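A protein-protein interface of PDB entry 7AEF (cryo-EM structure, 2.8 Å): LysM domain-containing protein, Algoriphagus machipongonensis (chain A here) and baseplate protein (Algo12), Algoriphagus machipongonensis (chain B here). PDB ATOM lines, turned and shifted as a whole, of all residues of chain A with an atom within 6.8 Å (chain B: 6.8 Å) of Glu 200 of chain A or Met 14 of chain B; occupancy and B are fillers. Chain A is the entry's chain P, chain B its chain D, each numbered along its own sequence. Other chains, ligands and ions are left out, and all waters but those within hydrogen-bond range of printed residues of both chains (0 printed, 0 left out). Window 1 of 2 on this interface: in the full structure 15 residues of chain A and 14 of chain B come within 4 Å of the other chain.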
ATOM      1  N   LYS A 196      -4.033  15.028  33.216  1.00  0.00           N
ATOM      2  CA  LYS A 196      -5.271  15.391  32.543  1.00  0.00           C
ATOM      3  C   LYS A 196      -5.078  15.805  31.093  1.00  0.00           C
ATOM      4  O   LYS A 196      -6.070  16.019  30.393  1.00  0.00           O
ATOM      5  CB  LYS A 196      -5.954  16.515  33.310  1.00  0.00           C
ATOM      6  CG  LYS A 196      -5.148  17.785  33.330  1.00  0.00           C
ATOM      7  CD  LYS A 196      -5.852  18.882  34.083  1.00  0.00           C
ATOM      8  CE  LYS A 196      -5.100  20.183  33.932  1.00  0.00           C
ATOM      9  NZ  LYS A 196      -5.857  21.332  34.480  1.00  0.00           N
ATOM     10  N   TYR A 197      -3.844  15.918  30.617  1.00  0.00           N
ATOM     11  CA  TYR A 197      -3.584  16.366  29.254  1.00  0.00           C
ATOM     12  C   TYR A 197      -3.476  15.231  28.248  1.00  0.00           C
ATOM     13  O   TYR A 197      -3.025  15.480  27.129  1.00  0.00           O
ATOM     14  CB  TYR A 197      -2.295  17.188  29.197  1.00  0.00           C
ATOM     15  CG  TYR A 197      -2.338  18.474  29.970  1.00  0.00           C
ATOM     16  CD1 TYR A 197      -3.112  19.537  29.540  1.00  0.00           C
ATOM     17  CD2 TYR A 197      -1.587  18.635  31.122  1.00  0.00           C
ATOM     18  CE1 TYR A 197      -3.147  20.716  30.239  1.00  0.00           C
ATOM     19  CE2 TYR A 197      -1.619  19.804  31.830  1.00  0.00           C
ATOM     20  CZ  TYR A 197      -2.399  20.844  31.382  1.00  0.00           C
ATOM     21  OH  TYR A 197      -2.432  22.022  32.080  1.00  0.00           O
ATOM     22  N   TYR A 198      -3.886  14.009  28.611  1.00  0.00           N
ATOM     23  CA  TYR A 198      -3.652  12.840  27.762  1.00  0.00           C
ATOM     24  C   TYR A 198      -4.469  12.870  26.472  1.00  0.00           C
ATOM     25  O   TYR A 198      -4.056  12.274  25.474  1.00  0.00           O
ATOM     26  CB  TYR A 198      -3.940  11.548  28.547  1.00  0.00           C
ATOM     27  CG  TYR A 198      -5.393  11.320  28.901  1.00  0.00           C
ATOM     28  CD1 TYR A 198      -5.954  11.918  30.018  1.00  0.00           C
ATOM     29  CD2 TYR A 198      -6.202  10.497  28.127  1.00  0.00           C
ATOM     30  CE1 TYR A 198      -7.274  11.721  30.343  1.00  0.00           C
ATOM     31  CE2 TYR A 198      -7.525  10.302  28.439  1.00  0.00           C
ATOM     32  CZ  TYR A 198      -8.055  10.912  29.553  1.00  0.00           C
ATOM     33  OH  TYR A 198      -9.370  10.719  29.880  1.00  0.00           O
ATOM     34  N   LEU A 199      -5.622  13.537  26.462  1.00  0.00           N
ATOM     35  CA  LEU A 199      -6.391  13.613  25.225  1.00  0.00           C
ATOM     36  C   LEU A 199      -5.848  14.656  24.263  1.00  0.00           C
ATOM     37  O   LEU A 199      -6.163  14.605  23.072  1.00  0.00           O
ATOM     38  CB  LEU A 199      -7.866  13.899  25.508  1.00  0.00           C
ATOM     39  CG  LEU A 199      -8.780  12.706  25.802  1.00  0.00           C
ATOM     40  CD1 LEU A 199     -10.219  13.152  25.929  1.00  0.00           C
ATOM     41  CD2 LEU A 199      -8.650  11.653  24.733  1.00  0.00           C
ATOM     42  N   GLU A 200      -5.047  15.606  24.740  1.00  0.00           N
ATOM     43  CA  GLU A 200      -4.420  16.555  23.827  1.00  0.00           C
ATOM     44  C   GLU A 200      -3.140  15.986  23.234  1.00  0.00           C
ATOM     45  O   GLU A 200      -2.752  16.358  22.123  1.00  0.00           O
ATOM     46  CB  GLU A 200      -4.143  17.869  24.549  1.00  0.00           C
ATOM     47  CG  GLU A 200      -5.377  18.582  25.036  1.00  0.00           C
ATOM     48  CD  GLU A 200      -6.290  19.001  23.906  1.00  0.00           C
ATOM     49  OE1 GLU A 200      -5.787  19.451  22.857  1.00  0.00           O
ATOM     50  OE2 GLU A 200      -7.524  18.883  24.069  1.00  0.00           O
ATOM     51  N   VAL A 201      -2.472  15.094  23.964  1.00  0.00           N
ATOM     52  CA  VAL A 201      -1.287  14.430  23.438  1.00  0.00           C
ATOM     53  C   VAL A 201      -1.685  13.418  22.372  1.00  0.00           C
ATOM     54  O   VAL A 201      -0.978  13.231  21.373  1.00  0.00           O
ATOM     55  CB  VAL A 201      -0.495  13.777  24.591  1.00  0.00           C
ATOM     56  CG1 VAL A 201       0.757  13.074  24.093  1.00  0.00           C
ATOM     57  CG2 VAL A 201      -0.127  14.814  25.621  1.00  0.00           C
ATOM     58  N   ALA A 202      -2.840  12.776  22.546  1.00  0.00           N
ATOM     59  CA  ALA A 202      -3.280  11.770  21.590  1.00  0.00           C
ATOM     60  C   ALA A 202      -3.786  12.407  20.303  1.00  0.00           C
ATOM     61  O   ALA A 202      -3.649  11.826  19.224  1.00  0.00           O
ATOM     62  CB  ALA A 202      -4.359  10.887  22.218  1.00  0.00           C
ATOM     63  N   LYS A 203      -4.366  13.605  20.396  1.00  0.00           N
ATOM     64  CA  LYS A 203      -4.842  14.294  19.206  1.00  0.00           C
ATOM     65  C   LYS A 203      -3.695  14.882  18.395  1.00  0.00           C
ATOM     66  O   LYS A 203      -3.791  14.998  17.171  1.00  0.00           O
ATOM     67  CB  LYS A 203      -5.819  15.399  19.599  1.00  0.00           C
ATOM     68  CG  LYS A 203      -7.264  15.012  19.498  1.00  0.00           C
ATOM     69  CD  LYS A 203      -8.147  16.204  19.775  1.00  0.00           C
ATOM     70  CE  LYS A 203      -8.115  16.575  21.236  1.00  0.00           C
ATOM     71  NZ  LYS A 203      -9.030  17.700  21.547  1.00  0.00           N
ATOM     72  N   ALA A 204      -2.606  15.266  19.059  1.00  0.00           N
ATOM     73  CA  ALA A 204      -1.474  15.844  18.349  1.00  0.00           C
ATOM     74  C   ALA A 204      -0.630  14.786  17.660  1.00  0.00           C
ATOM     75  O   ALA A 204       0.229  15.121  16.841  1.00  0.00           O
ATOM     76  CB  ALA A 204      -0.616  16.664  19.310  1.00  0.00           C
ATOM     77  N   ASN A 205      -0.864  13.514  17.964  1.00  0.00           N
ATOM     78  CA  ASN A 205      -0.132  12.406  17.371  1.00  0.00           C
ATOM     79  C   ASN A 205      -0.994  11.551  16.459  1.00  0.00           C
ATOM     80  O   ASN A 205      -0.487  10.594  15.866  1.00  0.00           O
ATOM     81  CB  ASN A 205       0.480  11.539  18.474  1.00  0.00           C
ATOM     82  CG  ASN A 205       1.651  12.206  19.152  1.00  0.00           C
ATOM     83  OD1 ASN A 205       2.782  12.107  18.693  1.00  0.00           O
ATOM     84  ND2 ASN A 205       1.387  12.892  20.248  1.00  0.00           N
ATOM     85  N   PRO A 222       3.888  18.490  22.746  1.00  0.00           N
ATOM     86  CA  PRO A 222       3.958  19.941  22.528  1.00  0.00           C
ATOM     87  C   PRO A 222       3.883  20.716  23.830  1.00  0.00           C
ATOM     88  O   PRO A 222       3.333  20.226  24.827  1.00  0.00           O
ATOM     89  CB  PRO A 222       2.725  20.216  21.650  1.00  0.00           C
ATOM     90  CG  PRO A 222       2.471  18.946  20.981  1.00  0.00           C
ATOM     91  CD  PRO A 222       2.780  17.895  21.990  1.00  0.00           C
ATOM     92  N   SER B   9       0.978  23.733  19.714  1.00  0.00           N
ATOM     93  CA  SER B   9       0.875  23.727  21.163  1.00  0.00           C
ATOM     94  C   SER B   9      -0.443  23.125  21.625  1.00  0.00           C
ATOM     95  O   SER B   9      -1.349  22.876  20.829  1.00  0.00           O
ATOM     96  CB  SER B   9       1.009  25.129  21.713  1.00  0.00           C
ATOM     97  OG  SER B   9      -0.054  25.929  21.272  1.00  0.00           O
ATOM     98  N   ILE B  10      -0.549  22.916  22.935  1.00  0.00           N
ATOM     99  CA  ILE B  10      -1.727  22.319  23.556  1.00  0.00           C
ATOM    100  C   ILE B  10      -2.357  23.267  24.573  1.00  0.00           C
ATOM    101  O   ILE B  10      -1.657  23.829  25.422  1.00  0.00           O
ATOM    102  CB  ILE B  10      -1.423  20.959  24.210  1.00  0.00           C
ATOM    103  CG1 ILE B  10      -0.408  21.109  25.340  1.00  0.00           C
ATOM    104  CG2 ILE B  10      -0.916  19.976  23.175  1.00  0.00           C
ATOM    105  CD1 ILE B  10      -0.068  19.848  26.042  1.00  0.00           C
ATOM    106  N   PRO B  11      -3.680  23.439  24.501  1.00  0.00           N
ATOM    107  CA  PRO B  11      -4.458  24.294  25.403  1.00  0.00           C
ATOM    108  C   PRO B  11      -4.290  23.870  26.843  1.00  0.00           C
ATOM    109  O   PRO B  11      -4.034  22.706  27.117  1.00  0.00           O
ATOM    110  CB  PRO B  11      -5.894  24.039  24.944  1.00  0.00           C
ATOM    111  CG  PRO B  11      -5.772  23.562  23.552  1.00  0.00           C
ATOM    112  CD  PRO B  11      -4.510  22.801  23.478  1.00  0.00           C
ATOM    113  N   LYS B  12      -4.415  24.833  27.764  1.00  0.00           N
ATOM    114  CA  LYS B  12      -4.260  24.562  29.197  1.00  0.00           C
ATOM    115  C   LYS B  12      -5.574  24.536  30.003  1.00  0.00           C
ATOM    116  O   LYS B  12      -5.587  24.141  31.178  1.00  0.00           O
ATOM    117  CB  LYS B  12      -3.289  25.580  29.817  1.00  0.00           C
ATOM    118  CG  LYS B  12      -2.977  25.369  31.298  1.00  0.00           C
ATOM    119  CD  LYS B  12      -2.033  26.354  31.851  1.00  0.00           C
ATOM    120  CE  LYS B  12      -1.765  26.095  33.325  1.00  0.00           C
ATOM    121  NZ  LYS B  12      -1.204  24.737  33.561  1.00  0.00           N
ATOM    122  N   ASP B  13      -6.703  24.893  29.408  1.00  0.00           N
ATOM    123  CA  ASP B  13      -7.975  24.878  30.135  1.00  0.00           C
ATOM    124  C   ASP B  13      -8.731  23.579  29.872  1.00  0.00           C
ATOM    125  O   ASP B  13      -9.704  23.528  29.120  1.00  0.00           O
ATOM    126  CB  ASP B  13      -8.825  26.077  29.747  1.00  0.00           C
ATOM    127  CG  ASP B  13     -10.022  26.265  30.665  1.00  0.00           C
ATOM    128  OD1 ASP B  13     -10.041  25.676  31.747  1.00  0.00           O
ATOM    129  OD2 ASP B  13     -10.914  27.040  30.324  1.00  0.00           O
ATOM    130  N   MET B  14      -8.285  22.512  30.522  1.00  0.00           N
ATOM    131  CA  MET B  14      -8.880  21.192  30.331  1.00  0.00           C
ATOM    132  C   MET B  14     -10.157  21.030  31.137  1.00  0.00           C
ATOM    133  O   MET B  14     -10.197  20.301  32.125  1.00  0.00           O
ATOM    134  CB  MET B  14      -7.900  20.103  30.724  1.00  0.00           C
ATOM    135  CG  MET B  14      -6.680  20.014  29.860  1.00  0.00           C
ATOM    136  SD  MET B  14      -7.068  19.564  28.173  1.00  0.00           S
ATOM    137  CE  MET B  14      -6.978  21.134  27.326  1.00  0.00           C
ATOM    138  N   SER B  15     -11.213  21.688  30.670  1.00  0.00           N
ATOM    139  CA  SER B  15     -12.511  21.654  31.336  1.00  0.00           C
ATOM    140  C   SER B  15     -13.625  21.831  30.321  1.00  0.00           C
ATOM    141  O   SER B  15     -13.662  22.835  29.606  1.00  0.00           O
ATOM    142  CB  SER B  15     -12.587  22.753  32.371  1.00  0.00           C
ATOM    143  OG  SER B  15     -13.853  22.778  32.976  1.00  0.00           O
ATOM    144  N   SER B  16     -14.525  20.869  30.233  1.00  0.00           N
ATOM    145  CA  SER B  16     -15.606  20.978  29.266  1.00  0.00           C
ATOM    146  C   SER B  16     -16.955  20.621  29.831  1.00  0.00           C
ATOM    147  O   SER B  16     -17.973  21.004  29.238  1.00  0.00           O
ATOM    148  CB  SER B  16     -15.334  20.082  28.070  1.00  0.00           C
ATOM    149  OG  SER B  16     -15.286  18.753  28.504  1.00  0.00           O
ATOM    150  N   ASP B  21     -14.412  14.955  29.634  1.00  0.00           N
ATOM    151  CA  ASP B  21     -13.867  15.513  30.871  1.00  0.00           C
ATOM    152  C   ASP B  21     -13.901  14.450  31.975  1.00  0.00           C
ATOM    153  O   ASP B  21     -14.948  14.207  32.580  1.00  0.00           O
ATOM    154  CB  ASP B  21     -14.687  16.770  31.169  1.00  0.00           C
ATOM    155  CG  ASP B  21     -14.271  17.553  32.383  1.00  0.00           C
ATOM    156  OD1 ASP B  21     -13.693  17.003  33.324  1.00  0.00           O
ATOM    157  OD2 ASP B  21     -14.590  18.764  32.399  1.00  0.00           O
ATOM    158  N   HIS B  23     -12.702  14.282  35.103  1.00  0.00           N
ATOM    159  CA  HIS B  23     -13.051  14.651  36.460  1.00  0.00           C
ATOM    160  C   HIS B  23     -14.525  14.934  36.587  1.00  0.00           C
ATOM    161  O   HIS B  23     -15.141  14.548  37.583  1.00  0.00           O
ATOM    162  CB  HIS B  23     -12.217  15.831  36.892  1.00  0.00           C
ATOM    163  CG  HIS B  23     -10.799  15.451  37.083  1.00  0.00           C
ATOM    164  ND1 HIS B  23     -10.391  14.621  38.101  1.00  0.00           N
ATOM    165  CD2 HIS B  23      -9.699  15.730  36.356  1.00  0.00           C
ATOM    166  CE1 HIS B  23      -9.091  14.424  38.005  1.00  0.00           C
ATOM    167  NE2 HIS B  23      -8.649  15.086  36.955  1.00  0.00           N
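The side-chain amino group (NZ) of Lys 203 of chain A is in salt-bridge range of the side-chain carboxylate (OE2) of Glu 200 of chain A.
Glu 200 of chain A touches just these residues of chain B: Pro 11 and Met 14.
Of the printed residues of chain B, Pro 222 of chain A touches Ser 9 (3.998 Å) and Ile 10 (3.6 Å).
Printed residues of chain A within 4 Å of Ser 9 of chain B: Pro 222.
Asp 21 of chain B touches none of the printed residues of chain A.
Among the printed residues, pairs that only touch across the chains: Tyr 197 of chain A with Pro 11 of chain B (3.8 Å), Tyr 197 of chain A with Met 14 of chain B (3.6 Å), Glu 200 of chain A with Pro 11 of chain B (3.6 Å), Glu 200 of chain A with Met 14 of chain B (3.7 Å), Pro 222 of chain A with Ser 9 of chain B (3.998 Å) and Pro 222 of chain A with Ile 10 of chain B (3.6 Å).
NZ of Lys 12 of chain B sits at hydrogen-bond distance from OH of Tyr 197 of chain A (3.3 Å).
Of the 11 printed residues of chain A, 3 touch a printed residue of chain B.
Hydrophobic or aromatic side chains of chain A within 4 Å of the printed part of chain B: Tyr 197 and Pro 222.
Along chain A the printed residues that touch a printed residue of chain B span positions 197 to 222.
Of the 10 printed residues of chain B, 5 touch a printed residue of chain A.
Hydrophobic or aromatic side chains of chain B within 4 Å of the printed part of chain A: Ile 10, Pro 11 and Met 14.
Among the printed residues, no Asp or Glu carboxylate lies within 4 Å of a Lys or Arg side-chain nitrogen of the other chain.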
